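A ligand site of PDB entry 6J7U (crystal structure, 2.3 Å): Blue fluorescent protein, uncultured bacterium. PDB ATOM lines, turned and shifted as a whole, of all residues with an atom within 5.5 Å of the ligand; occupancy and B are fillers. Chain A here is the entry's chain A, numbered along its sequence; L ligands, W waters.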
ATOM      1  N   THR A  25      -9.493 -17.713 -13.015  1.00  0.00           N
ATOM      2  CA  THR A  25      -9.315 -18.796 -12.039  1.00  0.00           C
ATOM      3  C   THR A  25     -10.282 -19.941 -12.309  1.00  0.00           C
ATOM      4  O   THR A  25     -11.455 -19.720 -12.665  1.00  0.00           O
ATOM      5  CB  THR A  25      -9.488 -18.297 -10.606  1.00  0.00           C
ATOM      6  OG1 THR A  25     -10.859 -17.971 -10.372  1.00  0.00           O
ATOM      7  CG2 THR A  25      -8.601 -17.052 -10.385  1.00  0.00           C
ATOM      8  N   GLY A  26      -9.841 -21.165 -12.086  1.00  0.00           N
ATOM      9  CA  GLY A  26     -10.760 -22.233 -12.379  1.00  0.00           C
ATOM     10  C   GLY A  26     -11.061 -22.421 -13.854  1.00  0.00           C
ATOM     11  O   GLY A  26     -12.219 -22.645 -14.226  1.00  0.00           O
ATOM     12  N   GLY A  27     -10.060 -22.270 -14.718  1.00  0.00           N
ATOM     13  CA  GLY A  27     -10.382 -22.372 -16.126  1.00  0.00           C
ATOM     14  C   GLY A  27     -10.351 -23.764 -16.692  1.00  0.00           C
ATOM     15  O   GLY A  27     -10.556 -23.969 -17.898  1.00  0.00           O
ATOM     16  N   SER A  28     -10.053 -24.765 -15.859  1.00  0.00           N
ATOM     17  CA  SER A  28      -9.872 -26.098 -16.431  1.00  0.00           C
ATOM     18  C   SER A  28     -11.193 -26.719 -16.863  1.00  0.00           C
ATOM     19  O   SER A  28     -11.184 -27.530 -17.800  1.00  0.00           O
ATOM     20  CB  SER A  28      -9.124 -26.990 -15.428  1.00  0.00           C
ATOM     21  OG  SER A  28      -9.728 -26.948 -14.146  1.00  0.00           O
ATOM     22  N   ARG A  29     -12.338 -26.345 -16.275  1.00  0.00           N
ATOM     23  CA  ARG A  29     -13.575 -27.010 -16.678  1.00  0.00           C
ATOM     24  C   ARG A  29     -14.812 -26.209 -16.282  1.00  0.00           C
ATOM     25  O   ARG A  29     -14.741 -25.143 -15.636  1.00  0.00           O
ATOM     26  CB  ARG A  29     -13.664 -28.419 -16.113  1.00  0.00           C
ATOM     27  CG  ARG A  29     -13.458 -28.496 -14.646  1.00  0.00           C
ATOM     28  CD  ARG A  29     -13.201 -29.941 -14.188  1.00  0.00           C
ATOM     29  NE  ARG A  29     -13.146 -29.930 -12.732  1.00  0.00           N
ATOM     30  CZ  ARG A  29     -14.194 -30.066 -11.922  1.00  0.00           C
ATOM     31  NH1 ARG A  29     -15.399 -30.327 -12.430  1.00  0.00           N
ATOM     32  NH2 ARG A  29     -14.045 -29.984 -10.601  1.00  0.00           N
ATOM     33  N   GLY A  30     -15.959 -26.714 -16.747  1.00  0.00           N
ATOM     34  CA  GLY A  30     -17.221 -26.079 -16.386  1.00  0.00           C
ATOM     35  C   GLY A  30     -17.319 -24.666 -16.912  1.00  0.00           C
ATOM     36  O   GLY A  30     -16.832 -24.343 -17.986  1.00  0.00           O
ATOM     37  N   ILE A  31     -17.892 -23.775 -16.108  1.00  0.00           N
ATOM     38  CA  ILE A  31     -18.054 -22.390 -16.546  1.00  0.00           C
ATOM     39  C   ILE A  31     -16.692 -21.752 -16.883  1.00  0.00           C
ATOM     40  O   ILE A  31     -16.568 -21.013 -17.873  1.00  0.00           O
ATOM     41  CB  ILE A  31     -18.809 -21.621 -15.481  1.00  0.00           C
ATOM     42  CG1 ILE A  31     -20.205 -22.222 -15.322  1.00  0.00           C
ATOM     43  CG2 ILE A  31     -18.914 -20.167 -15.858  1.00  0.00           C
ATOM     44  CD1 ILE A  31     -20.890 -21.756 -14.078  1.00  0.00           C
ATOM     45  N   GLY A  32     -15.644 -22.076 -16.117  1.00  0.00           N
ATOM     46  CA  GLY A  32     -14.375 -21.407 -16.359  1.00  0.00           C
ATOM     47  C   GLY A  32     -13.727 -21.805 -17.680  1.00  0.00           C
ATOM     48  O   GLY A  32     -13.151 -20.963 -18.380  1.00  0.00           O
ATOM     49  N   THR A  49      -6.129 -20.990 -14.053  1.00  0.00           N
ATOM     50  CA  THR A  49      -5.628 -21.837 -12.997  1.00  0.00           C
ATOM     51  C   THR A  49      -6.504 -23.072 -12.859  1.00  0.00           C
ATOM     52  O   THR A  49      -7.628 -23.116 -13.343  1.00  0.00           O
ATOM     53  CB  THR A  49      -5.567 -21.070 -11.662  1.00  0.00           C
ATOM     54  OG1 THR A  49      -6.914 -20.823 -11.212  1.00  0.00           O
ATOM     55  CG2 THR A  49      -4.838 -19.747 -11.846  1.00  0.00           C
ATOM     56  N   TYR A  50      -5.919 -24.076 -12.199  1.00  0.00           N
ATOM     57  CA  TYR A  50      -6.599 -25.290 -11.781  1.00  0.00           C
ATOM     58  C   TYR A  50      -5.908 -25.751 -10.500  1.00  0.00           C
ATOM     59  O   TYR A  50      -4.763 -25.381 -10.228  1.00  0.00           O
ATOM     60  CB  TYR A  50      -6.559 -26.390 -12.880  1.00  0.00           C
ATOM     61  CG  TYR A  50      -5.157 -26.910 -13.136  1.00  0.00           C
ATOM     62  CD1 TYR A  50      -4.251 -26.188 -13.880  1.00  0.00           C
ATOM     63  CD2 TYR A  50      -4.755 -28.139 -12.649  1.00  0.00           C
ATOM     64  CE1 TYR A  50      -2.960 -26.633 -14.089  1.00  0.00           C
ATOM     65  CE2 TYR A  50      -3.457 -28.619 -12.882  1.00  0.00           C
ATOM     66  CZ  TYR A  50      -2.569 -27.845 -13.592  1.00  0.00           C
ATOM     67  OH  TYR A  50      -1.261 -28.274 -13.827  1.00  0.00           O
ATOM     68  N   VAL A  51      -6.615 -26.564  -9.723  1.00  0.00           N
ATOM     69  CA  VAL A  51      -6.091 -27.096  -8.477  1.00  0.00           C
ATOM     70  C   VAL A  51      -5.889 -28.621  -8.547  1.00  0.00           C
ATOM     71  O   VAL A  51      -4.849 -29.136  -8.157  1.00  0.00           O
ATOM     72  CB  VAL A  51      -6.993 -26.718  -7.297  1.00  0.00           C
ATOM     73  CG1 VAL A  51      -8.453 -26.784  -7.740  1.00  0.00           C
ATOM     74  CG2 VAL A  51      -6.680 -27.623  -6.084  1.00  0.00           C
ATOM     75  N   SER A  52      -6.929 -29.353  -8.942  1.00  0.00           N
ATOM     76  CA  SER A  52      -6.908 -30.808  -8.800  1.00  0.00           C
ATOM     77  C   SER A  52      -5.882 -31.453  -9.714  1.00  0.00           C
ATOM     78  O   SER A  52      -5.771 -31.136 -10.893  1.00  0.00           O
ATOM     79  CB  SER A  52      -8.290 -31.405  -9.074  1.00  0.00           C
ATOM     80  OG  SER A  52      -9.301 -30.642  -8.428  1.00  0.00           O
ATOM     81  N   SER A  55      -7.169 -32.706 -12.883  1.00  0.00           N
ATOM     82  CA  SER A  55      -7.385 -31.734 -13.941  1.00  0.00           C
ATOM     83  C   SER A  55      -6.133 -31.366 -14.721  1.00  0.00           C
ATOM     84  O   SER A  55      -6.213 -30.517 -15.613  1.00  0.00           O
ATOM     85  CB  SER A  55      -7.993 -30.441 -13.383  1.00  0.00           C
ATOM     86  OG  SER A  55      -9.286 -30.653 -12.847  1.00  0.00           O
ATOM     87  N   ALA A  78      -2.693 -23.677  -9.006  1.00  0.00           N
ATOM     88  CA  ALA A  78      -2.749 -22.738  -7.889  1.00  0.00           C
ATOM     89  C   ALA A  78      -4.015 -23.064  -7.124  1.00  0.00           C
ATOM     90  O   ALA A  78      -5.108 -22.896  -7.688  1.00  0.00           O
ATOM     91  CB  ALA A  78      -2.797 -21.297  -8.372  1.00  0.00           C
ATOM     92  N   ASP A  79      -3.889 -23.528  -5.887  1.00  0.00           N
ATOM     93  CA  ASP A  79      -5.026 -23.802  -5.008  1.00  0.00           C
ATOM     94  C   ASP A  79      -5.596 -22.482  -4.494  1.00  0.00           C
ATOM     95  O   ASP A  79      -4.917 -21.740  -3.778  1.00  0.00           O
ATOM     96  CB  ASP A  79      -4.560 -24.681  -3.855  1.00  0.00           C
ATOM     97  CG  ASP A  79      -5.707 -25.120  -2.938  1.00  0.00           C
ATOM     98  OD1 ASP A  79      -6.802 -24.463  -2.915  1.00  0.00           O
ATOM     99  OD2 ASP A  79      -5.494 -26.108  -2.200  1.00  0.00           O
ATOM    100  N   SER A  80      -6.860 -22.203  -4.838  1.00  0.00           N
ATOM    101  CA  SER A  80      -7.505 -20.990  -4.343  1.00  0.00           C
ATOM    102  C   SER A  80      -7.614 -20.988  -2.839  1.00  0.00           C
ATOM    103  O   SER A  80      -7.723 -19.918  -2.248  1.00  0.00           O
ATOM    104  CB  SER A  80      -8.921 -20.827  -4.878  1.00  0.00           C
ATOM    105  OG  SER A  80      -8.932 -20.439  -6.221  1.00  0.00           O
ATOM    106  N   ALA A  81      -7.590 -22.166  -2.205  1.00  0.00           N
ATOM    107  CA  ALA A  81      -7.577 -22.189  -0.751  1.00  0.00           C
ATOM    108  C   ALA A  81      -6.342 -21.464  -0.207  1.00  0.00           C
ATOM    109  O   ALA A  81      -6.383 -20.880   0.886  1.00  0.00           O
ATOM    110  CB  ALA A  81      -7.676 -23.644  -0.295  1.00  0.00           C
ATOM    111  N   ASN A 106     -13.606 -16.983 -11.151  1.00  0.00           N
ATOM    112  CA  ASN A 106     -14.609 -18.022 -11.376  1.00  0.00           C
ATOM    113  C   ASN A 106     -14.518 -19.227 -10.451  1.00  0.00           C
ATOM    114  O   ASN A 106     -15.540 -19.855 -10.183  1.00  0.00           O
ATOM    115  CB  ASN A 106     -14.506 -18.542 -12.806  1.00  0.00           C
ATOM    116  CG  ASN A 106     -15.201 -19.865 -12.975  1.00  0.00           C
ATOM    117  OD1 ASN A 106     -16.405 -19.920 -13.111  1.00  0.00           O
ATOM    118  ND2 ASN A 106     -14.445 -20.936 -12.939  1.00  0.00           N
ATOM    119  N   ALA A 107     -13.322 -19.632 -10.032  1.00  0.00           N
ATOM    120  CA  ALA A 107     -13.206 -20.833  -9.219  1.00  0.00           C
ATOM    121  C   ALA A 107     -14.043 -20.695  -7.942  1.00  0.00           C
ATOM    122  O   ALA A 107     -13.994 -19.665  -7.263  1.00  0.00           O
ATOM    123  CB  ALA A 107     -11.741 -21.089  -8.890  1.00  0.00           C
ATOM    124  N   GLY A 108     -14.775 -21.745  -7.580  1.00  0.00           N
ATOM    125  CA  GLY A 108     -15.656 -21.680  -6.428  1.00  0.00           C
ATOM    126  C   GLY A 108     -15.866 -23.052  -5.822  1.00  0.00           C
ATOM    127  O   GLY A 108     -15.526 -24.071  -6.422  1.00  0.00           O
ATOM    128  N   ILE A 109     -16.387 -23.061  -4.612  1.00  0.00           N
ATOM    129  CA  ILE A 109     -16.726 -24.304  -3.947  1.00  0.00           C
ATOM    130  C   ILE A 109     -18.111 -24.146  -3.336  1.00  0.00           C
ATOM    131  O   ILE A 109     -18.520 -23.048  -2.943  1.00  0.00           O
ATOM    132  CB  ILE A 109     -15.686 -24.730  -2.868  1.00  0.00           C
ATOM    133  CG1 ILE A 109     -15.951 -26.155  -2.444  1.00  0.00           C
ATOM    134  CG2 ILE A 109     -15.761 -23.843  -1.654  1.00  0.00           C
ATOM    135  CD1 ILE A 109     -14.966 -26.720  -1.389  1.00  0.00           C
ATOM    136  N   ARG A 125     -12.645 -22.946   4.386  1.00  0.00           N
ATOM    137  CA  ARG A 125     -12.406 -23.347   3.008  1.00  0.00           C
ATOM    138  C   ARG A 125     -13.307 -22.581   2.039  1.00  0.00           C
ATOM    139  O   ARG A 125     -12.854 -22.118   0.985  1.00  0.00           O
ATOM    140  CB  ARG A 125     -12.635 -24.841   2.879  1.00  0.00           C
ATOM    141  CG  ARG A 125     -11.958 -25.475   1.717  1.00  0.00           C
ATOM    142  CD  ARG A 125     -12.084 -27.015   1.675  1.00  0.00           C
ATOM    143  NE  ARG A 125     -11.600 -27.420   0.357  1.00  0.00           N
ATOM    144  CZ  ARG A 125     -10.293 -27.554   0.068  1.00  0.00           C
ATOM    145  NH1 ARG A 125      -9.376 -27.360   1.024  1.00  0.00           N
ATOM    146  NH2 ARG A 125      -9.900 -27.894  -1.158  1.00  0.00           N
ATOM    147  N   ILE A 129     -11.726 -19.728  -0.570  1.00  0.00           N
ATOM    148  CA  ILE A 129     -11.840 -20.003  -1.994  1.00  0.00           C
ATOM    149  C   ILE A 129     -12.798 -19.034  -2.645  1.00  0.00           C
ATOM    150  O   ILE A 129     -12.556 -18.539  -3.766  1.00  0.00           O
ATOM    151  CB  ILE A 129     -12.292 -21.457  -2.240  1.00  0.00           C
ATOM    152  CG1 ILE A 129     -11.269 -22.461  -1.774  1.00  0.00           C
ATOM    153  CG2 ILE A 129     -12.628 -21.694  -3.735  1.00  0.00           C
ATOM    154  CD1 ILE A 129     -11.779 -23.854  -1.976  1.00  0.00           C
ATOM    155  N   ASN A 130     -13.942 -18.787  -2.014  1.00  0.00           N
ATOM    156  CA  ASN A 130     -14.957 -17.979  -2.673  1.00  0.00           C
ATOM    157  C   ASN A 130     -14.786 -16.505  -2.433  1.00  0.00           C
ATOM    158  O   ASN A 130     -15.373 -15.720  -3.175  1.00  0.00           O
ATOM    159  CB  ASN A 130     -16.368 -18.373  -2.213  1.00  0.00           C
ATOM    160  CG  ASN A 130     -16.738 -19.747  -2.642  1.00  0.00           C
ATOM    161  OD1 ASN A 130     -15.957 -20.389  -3.357  1.00  0.00           O
ATOM    162  ND2 ASN A 130     -17.860 -20.245  -2.159  1.00  0.00           N
ATOM    163  N   ILE A 154     -17.507 -14.174 -10.567  1.00  0.00           N
ATOM    164  CA  ILE A 154     -18.627 -15.101 -10.721  1.00  0.00           C
ATOM    165  C   ILE A 154     -19.285 -15.296  -9.334  1.00  0.00           C
ATOM    166  O   ILE A 154     -18.682 -15.819  -8.391  1.00  0.00           O
ATOM    167  CB  ILE A 154     -18.187 -16.416 -11.357  1.00  0.00           C
ATOM    168  CG1 ILE A 154     -17.557 -16.197 -12.726  1.00  0.00           C
ATOM    169  CG2 ILE A 154     -19.346 -17.298 -11.572  1.00  0.00           C
ATOM    170  CD1 ILE A 154     -18.387 -15.311 -13.671  1.00  0.00           C
ATOM    171  N   GLY A 155     -20.509 -14.826  -9.204  1.00  0.00           N
ATOM    172  CA  GLY A 155     -21.249 -14.961  -7.966  1.00  0.00           C
ATOM    173  C   GLY A 155     -22.183 -16.149  -7.947  1.00  0.00           C
ATOM    174  O   GLY A 155     -21.761 -17.298  -8.123  1.00  0.00           O
ATOM    175  N   SER A 156     -23.448 -15.913  -7.649  1.00  0.00           N
ATOM    176  CA  SER A 156     -24.449 -16.964  -7.687  1.00  0.00           C
ATOM    177  C   SER A 156     -25.804 -16.334  -7.376  1.00  0.00           C
ATOM    178  O   SER A 156     -25.887 -15.389  -6.572  1.00  0.00           O
ATOM    179  CB  SER A 156     -24.124 -18.056  -6.666  1.00  0.00           C
ATOM    180  OG  SER A 156     -25.257 -18.885  -6.403  1.00  0.00           O
ATOM    181  N   CYS A 157     -26.857 -16.926  -7.953  1.00  0.00           N
ATOM    182  CA  CYS A 157     -28.210 -16.490  -7.628  1.00  0.00           C
ATOM    183  C   CYS A 157     -28.499 -16.654  -6.125  1.00  0.00           C
ATOM    184  O   CYS A 157     -29.251 -15.851  -5.560  1.00  0.00           O
ATOM    185  CB  CYS A 157     -29.246 -17.257  -8.486  1.00  0.00           C
ATOM    186  SG  CYS A 157     -29.330 -19.069  -8.226  1.00  0.00           S
ATOM    187  N   TYR A 170     -22.636 -21.042   1.935  1.00  0.00           N
ATOM    188  CA  TYR A 170     -22.363 -20.707   0.565  1.00  0.00           C
ATOM    189  C   TYR A 170     -22.981 -19.364   0.216  1.00  0.00           C
ATOM    190  O   TYR A 170     -22.314 -18.495  -0.370  1.00  0.00           O
ATOM    191  CB  TYR A 170     -22.876 -21.815  -0.359  1.00  0.00           C
ATOM    192  CG  TYR A 170     -22.709 -21.545  -1.836  1.00  0.00           C
ATOM    193  CD1 TYR A 170     -21.528 -21.844  -2.487  1.00  0.00           C
ATOM    194  CD2 TYR A 170     -23.758 -20.997  -2.574  1.00  0.00           C
ATOM    195  CE1 TYR A 170     -21.358 -21.604  -3.849  1.00  0.00           C
ATOM    196  CE2 TYR A 170     -23.615 -20.731  -3.940  1.00  0.00           C
ATOM    197  CZ  TYR A 170     -22.418 -21.049  -4.591  1.00  0.00           C
ATOM    198  OH  TYR A 170     -22.283 -20.826  -5.954  1.00  0.00           O
ATOM    199  N   LYS A 174     -21.002 -15.863  -1.219  1.00  0.00           N
ATOM    200  CA  LYS A 174     -21.285 -15.273  -2.510  1.00  0.00           C
ATOM    201  C   LYS A 174     -21.866 -13.871  -2.386  1.00  0.00           C
ATOM    202  O   LYS A 174     -21.629 -13.061  -3.259  1.00  0.00           O
ATOM    203  CB  LYS A 174     -22.190 -16.187  -3.320  1.00  0.00           C
ATOM    204  CG  LYS A 174     -21.505 -17.507  -3.873  1.00  0.00           C
ATOM    205  CD  LYS A 174     -20.288 -17.207  -4.724  1.00  0.00           C
ATOM    206  CE  LYS A 174     -19.832 -18.454  -5.540  1.00  0.00           C
ATOM    207  NZ  LYS A 174     -18.887 -18.039  -6.611  1.00  0.00           N
ATOM    208  N   PRO A 200     -24.896 -16.816 -11.914  1.00  0.00           N
ATOM    209  CA  PRO A 200     -25.570 -17.934 -12.567  1.00  0.00           C
ATOM    210  C   PRO A 200     -26.779 -18.403 -11.777  1.00  0.00           C
ATOM    211  O   PRO A 200     -26.780 -18.397 -10.546  1.00  0.00           O
ATOM    212  CB  PRO A 200     -24.484 -19.012 -12.623  1.00  0.00           C
ATOM    213  CG  PRO A 200     -23.182 -18.299 -12.258  1.00  0.00           C
ATOM    214  CD  PRO A 200     -23.590 -17.205 -11.359  1.00  0.00           C
ATOM    215  N   GLY A 201     -27.800 -18.857 -12.522  1.00  0.00           N
ATOM    216  CA  GLY A 201     -28.834 -19.716 -11.996  1.00  0.00           C
ATOM    217  C   GLY A 201     -28.323 -21.125 -12.148  1.00  0.00           C
ATOM    218  O   GLY A 201     -27.122 -21.312 -12.336  1.00  0.00           O
ATOM    219  N   PRO A 202     -29.167 -22.146 -12.112  1.00  0.00           N
ATOM    220  CA  PRO A 202     -28.642 -23.516 -12.293  1.00  0.00           C
ATOM    221  C   PRO A 202     -28.017 -23.652 -13.678  1.00  0.00           C
ATOM    222  O   PRO A 202     -28.669 -23.360 -14.686  1.00  0.00           O
ATOM    223  CB  PRO A 202     -29.889 -24.404 -12.177  1.00  0.00           C
ATOM    224  CG  PRO A 202     -31.021 -23.463 -11.846  1.00  0.00           C
ATOM    225  CD  PRO A 202     -30.632 -22.102 -12.241  1.00  0.00           C
ATOM    226  N   ILE A 203     -26.783 -24.155 -13.720  1.00  0.00           N
ATOM    227  CA  ILE A 203     -26.013 -24.316 -14.963  1.00  0.00           C
ATOM    228  C   ILE A 203     -25.480 -25.753 -15.008  1.00  0.00           C
ATOM    229  O   ILE A 203     -24.808 -26.209 -14.067  1.00  0.00           O
ATOM    230  CB  ILE A 203     -24.835 -23.325 -15.087  1.00  0.00           C
ATOM    231  CG1 ILE A 203     -25.249 -21.873 -14.978  1.00  0.00           C
ATOM    232  CG2 ILE A 203     -24.280 -23.382 -16.465  1.00  0.00           C
ATOM    233  CD1 ILE A 203     -26.083 -21.491 -16.161  1.00  0.00           C
ATOM    234  N   THR A 205     -23.326 -28.387 -15.018  1.00  0.00           N
ATOM    235  CA  THR A 205     -21.896 -28.705 -14.893  1.00  0.00           C
ATOM    236  C   THR A 205     -21.736 -29.838 -13.866  1.00  0.00           C
ATOM    237  O   THR A 205     -22.713 -30.347 -13.292  1.00  0.00           O
ATOM    238  CB  THR A 205     -21.053 -27.505 -14.451  1.00  0.00           C
ATOM    239  OG1 THR A 205     -21.303 -27.234 -13.070  1.00  0.00           O
ATOM    240  CG2 THR A 205     -21.315 -26.285 -15.295  1.00  0.00           C
ATOM    241  N   ASP A 206     -20.480 -30.198 -13.596  1.00  0.00           N
ATOM    242  CA  ASP A 206     -20.239 -31.257 -12.619  1.00  0.00           C
ATOM    243  C   ASP A 206     -20.687 -30.841 -11.224  1.00  0.00           C
ATOM    244  O   ASP A 206     -21.230 -31.659 -10.464  1.00  0.00           O
ATOM    245  CB  ASP A 206     -18.772 -31.666 -12.637  1.00  0.00           C
ATOM    246  CG  ASP A 206     -18.378 -32.249 -13.964  1.00  0.00           C
ATOM    247  OD1 ASP A 206     -19.287 -32.762 -14.661  1.00  0.00           O
ATOM    248  OD2 ASP A 206     -17.183 -32.177 -14.315  1.00  0.00           O
ATOM    249  N   MET A 207     -20.474 -29.575 -10.868  1.00  0.00           N
ATOM    250  CA  MET A 207     -20.919 -29.133  -9.556  1.00  0.00           C
ATOM    251  C   MET A 207     -22.448 -29.192  -9.448  1.00  0.00           C
ATOM    252  O   MET A 207     -22.979 -29.503  -8.374  1.00  0.00           O
ATOM    253  CB  MET A 207     -20.372 -27.717  -9.307  1.00  0.00           C
ATOM    254  CG  MET A 207     -20.600 -27.086  -7.927  1.00  0.00           C
ATOM    255  SD  MET A 207     -22.021 -25.977  -7.782  1.00  0.00           S
ATOM    256  CE  MET A 207     -21.250 -24.407  -8.165  1.00  0.00           C
ATOM    257  N   ASN A 208     -23.178 -28.934 -10.543  1.00  0.00           N
ATOM    258  CA  ASN A 208     -24.647 -28.972 -10.546  1.00  0.00           C
ATOM    259  C   ASN A 208     -25.217 -29.688 -11.765  1.00  0.00           C
ATOM    260  O   ASN A 208     -25.741 -29.050 -12.688  1.00  0.00           O
ATOM    261  CB  ASN A 208     -25.198 -27.551 -10.452  1.00  0.00           C
ATOM    262  CG  ASN A 208     -26.654 -27.536 -10.085  1.00  0.00           C
ATOM    263  OD1 ASN A 208     -27.247 -28.576  -9.770  1.00  0.00           O
ATOM    264  ND2 ASN A 208     -27.245 -26.350 -10.061  1.00  0.00           N
HETATM  265  P1  LIG L   1     -17.309 -26.806 -11.303  1.00  0.00           P
HETATM  266  O1  LIG L   1     -17.115 -27.388  -9.937  1.00  0.00           O
HETATM  267  O2  LIG L   1     -18.132 -27.514 -12.340  1.00  0.00           O
HETATM  268  O3  LIG L   1     -15.863 -26.396 -11.977  1.00  0.00           O
HETATM  269  C1  LIG L   1     -15.056 -25.951 -10.881  1.00  0.00           C
HETATM  270  C2  LIG L   1     -13.811 -25.210 -11.420  1.00  0.00           C
HETATM  271  O4  LIG L   1     -13.292 -24.391 -10.397  1.00  0.00           O
HETATM  272  C3  LIG L   1     -12.739 -26.283 -11.874  1.00  0.00           C
HETATM  273  O5  LIG L   1     -11.972 -25.842 -12.995  1.00  0.00           O
HETATM  274  C4  LIG L   1     -11.839 -26.330 -10.661  1.00  0.00           C
HETATM  275  O6  LIG L   1     -10.550 -26.578 -10.951  1.00  0.00           O
HETATM  276  C5  LIG L   1     -11.983 -24.825 -10.104  1.00  0.00           C
HETATM  277  N1  LIG L   1     -11.720 -24.831  -8.621  1.00  0.00           N
HETATM  278  C6  LIG L   1     -12.503 -25.341  -7.535  1.00  0.00           C
HETATM  279  N2  LIG L   1     -11.893 -25.217  -6.339  1.00  0.00           N
HETATM  280  C7  LIG L   1     -10.672 -24.609  -6.656  1.00  0.00           C
HETATM  281  C8  LIG L   1      -9.605 -24.214  -5.869  1.00  0.00           C
HETATM  282  N3  LIG L   1      -9.662 -24.421  -4.513  1.00  0.00           N
HETATM  283  N4  LIG L   1      -8.474 -23.628  -6.411  1.00  0.00           N
HETATM  284  C9  LIG L   1      -8.488 -23.462  -7.792  1.00  0.00           C
HETATM  285  N5  LIG L   1      -9.448 -23.782  -8.695  1.00  0.00           N
HETATM  286  C10 LIG L   1     -10.551 -24.375  -8.077  1.00  0.00           C
HETATM  287  O7  LIG L   1     -17.992 -25.314 -10.826  1.00  0.00           O
HETATM  288  P2  LIG L   1     -18.914 -24.641 -11.970  1.00  0.00           P
HETATM  289  O8  LIG L   1     -18.250 -24.565 -13.291  1.00  0.00           O
HETATM  290  O9  LIG L   1     -20.345 -25.112 -11.805  1.00  0.00           O
HETATM  291  O10 LIG L   1     -19.134 -22.875 -11.589  1.00  0.00           O
HETATM  292  C11 LIG L   1     -17.991 -22.289 -11.133  1.00  0.00           C
HETATM  293  C12 LIG L   1     -18.369 -20.962 -10.465  1.00  0.00           C
HETATM  294  O11 LIG L   1     -19.780 -20.661 -10.671  1.00  0.00           O
HETATM  295  C13 LIG L   1     -18.207 -21.090  -8.880  1.00  0.00           C
HETATM  296  O12 LIG L   1     -17.814 -19.889  -8.374  1.00  0.00           O
HETATM  297  C14 LIG L   1     -19.607 -21.411  -8.439  1.00  0.00           C
HETATM  298  O13 LIG L   1     -19.807 -21.049  -7.134  1.00  0.00           O
HETATM  299  C15 LIG L   1     -20.406 -20.474  -9.395  1.00  0.00           C
HETATM  300  N6  LIG L   1     -21.830 -20.844  -9.498  1.00  0.00           N
HETATM  301  C16 LIG L   1     -22.203 -21.981 -10.153  1.00  0.00           C
HETATM  302  C17 LIG L   1     -23.511 -22.394 -10.150  1.00  0.00           C
HETATM  303  C18 LIG L   1     -23.844 -23.566 -10.946  1.00  0.00           C
HETATM  304  O14 LIG L   1     -24.958 -24.030 -10.975  1.00  0.00           O
HETATM  305  N7  LIG L   1     -22.902 -24.172 -11.778  1.00  0.00           N
HETATM  306  C19 LIG L   1     -24.597 -21.633  -9.370  1.00  0.00           C
HETATM  307  C20 LIG L   1     -24.143 -20.291  -8.942  1.00  0.00           C
HETATM  308  C21 LIG L   1     -22.846 -19.947  -9.015  1.00  0.00           C
HETATM  309  P3  LIG L   1     -10.173 -28.370 -11.081  1.00  0.00           P
HETATM  310  O15 LIG L   1     -10.884 -28.823  -9.831  1.00  0.00           O
HETATM  311  O16 LIG L   1     -10.764 -28.787 -12.434  1.00  0.00           O
HETATM  312  O17 LIG L   1      -8.690 -28.218 -11.019  1.00  0.00           O
HETATM  313  O   HOH W   1     -15.863 -23.615 -13.669  1.00  0.00           O
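The backbone NH (N) of Asn 106 is in hydrogen-bond range of the side-chain hydroxyl (OG1) of Thr 25 (3.0 Å). The backbone NH (N) of Ala 78 is in hydrogen-bond range of the backbone carbonyl oxygen (O) of Tyr 50. The backbone NH (N) of Met 207 lies close to the side-chain hydroxyl (OG1) of Thr 205 (3.3 Å). The guanidinium group of Arg 29 is in salt-bridge range of the side-chain carboxylate of Asp 206 (3.2 Å). The backbone NH (N) of Gly 26 sits at hydrogen-bond distance from the side-chain hydroxyl (OG1) of Thr 49 (3.1 Å). The side-chain amino group of Lys 174 sits at hydrogen-bond distance from the backbone carbonyl oxygen of Ile 154 (2.9 Å). The side-chain amide nitrogen of Asn 106 is in hydrogen-bond range of the backbone carbonyl oxygen of Gly 26, 3.1 Å away. The side-chain amino group (NZ) of Lys 174 lies within hydrogen-bond range of the backbone carbonyl oxygen (O) of Gly 155 (3.3 Å).
The guanidinium group of Arg 29 is in salt-bridge range of an oxygen (O16) of the ligand, 2.7 Å away. A nitrogen (N3) of the ligand lies within hydrogen-bond range of the side-chain carboxylate of Asp 79 (3.3 Å). The backbone carbonyl oxygen (O) of Asn 106 is in hydrogen-bond range of an oxygen (O12) of the ligand, 2.9 Å away. The side-chain hydroxyl (OG) of Ser 52 is in hydrogen-bond range of an oxygen (O15) of the ligand, at 2.8 Å. N of Arg 29 sits at hydrogen-bond distance from O5 of the ligand, 3.3 Å away. OG of Ser 55 lies within hydrogen-bond range of O16 of the ligand (2.4 Å). An oxygen (O5) of the ligand is in hydrogen-bond range of the backbone carbonyl oxygen (O) of Gly 26. The backbone NH (N) of Met 207 lies within hydrogen-bond range of an oxygen (O2) of the ligand (3.4 Å). An oxygen (O14) of the ligand is in hydrogen-bond range of the backbone NH (N) of Ile 203. N4 of the ligand lies within hydrogen-bond range of N of Ser 80 (2.7 Å). The backbone NH of Ser 52 sits at hydrogen-bond distance from an oxygen (O17) of the ligand (3.0 Å). An oxygen (O17) of the ligand is in hydrogen-bond range of the backbone NH (N) of Val 51, 3.0 Å away. O12 of the ligand lies within hydrogen-bond range of NZ of Lys 174, 2.8 Å away. The side-chain amide nitrogen (ND2) of Asn 208 is in hydrogen-bond range of an oxygen (O14) of the ligand, at 3.4 Å. O8 of the ligand lies within hydrogen-bond range of N of Ile 31. The side-chain hydroxyl of Ser 80 sits close to a nitrogen (N4) of the ligand (3.2 Å). OG of Ser 28 is in hydrogen-bond range of O16 of the ligand, 2.7 Å away. OG1 of Thr 205 lies within hydrogen-bond range of O9 of the ligand, 2.6 Å away. O13 of the ligand is in hydrogen-bond range of OH of Tyr 170 (2.8 Å).
Gly 30 touches the ligand. Tyr 50 touches the ligand (CB to O17, 3.4 Å). Ala 78 touches the ligand (O to C9, 3.4 Å). N of Ala 81 touches N3 of the ligand (3.8 Å). CB of Ala 107 touches N5 of the ligand, 3.5 Å away. Gly 108 touches the ligand. CD1 of Ile 129 touches N3 of the ligand, at 3.4 Å. CG2 of Ile 154 touches O11 of the ligand, at 3.5 Å. Gly 155 touches the ligand. Ser 156 touches the ligand. Pro 200 touches the ligand. Gly 201 touches the ligand. Pro 202 touches the ligand. Asp 206 touches the ligand (N to O2, 3.8 Å). 30 residues have an atom within 4 Å of the ligand: Gly 26, Ser 28, Arg 29, Gly 30, Ile 31, Tyr 50, Val 51, Ser 52, Ser 55, Ala 78, Asp 79, Ser 80, Ala 81, Asn 106, Ala 107, Gly 108, Ile 129, Ile 154, Gly 155, Ser 156, Tyr 170, Lys 174, Pro 200, Gly 201, Pro 202, Ile 203, Thr 205, Asp 206, Met 207 and Asn 208. The nearest printed residue that does not touch the ligand is Gly 27 (4.4 Å).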
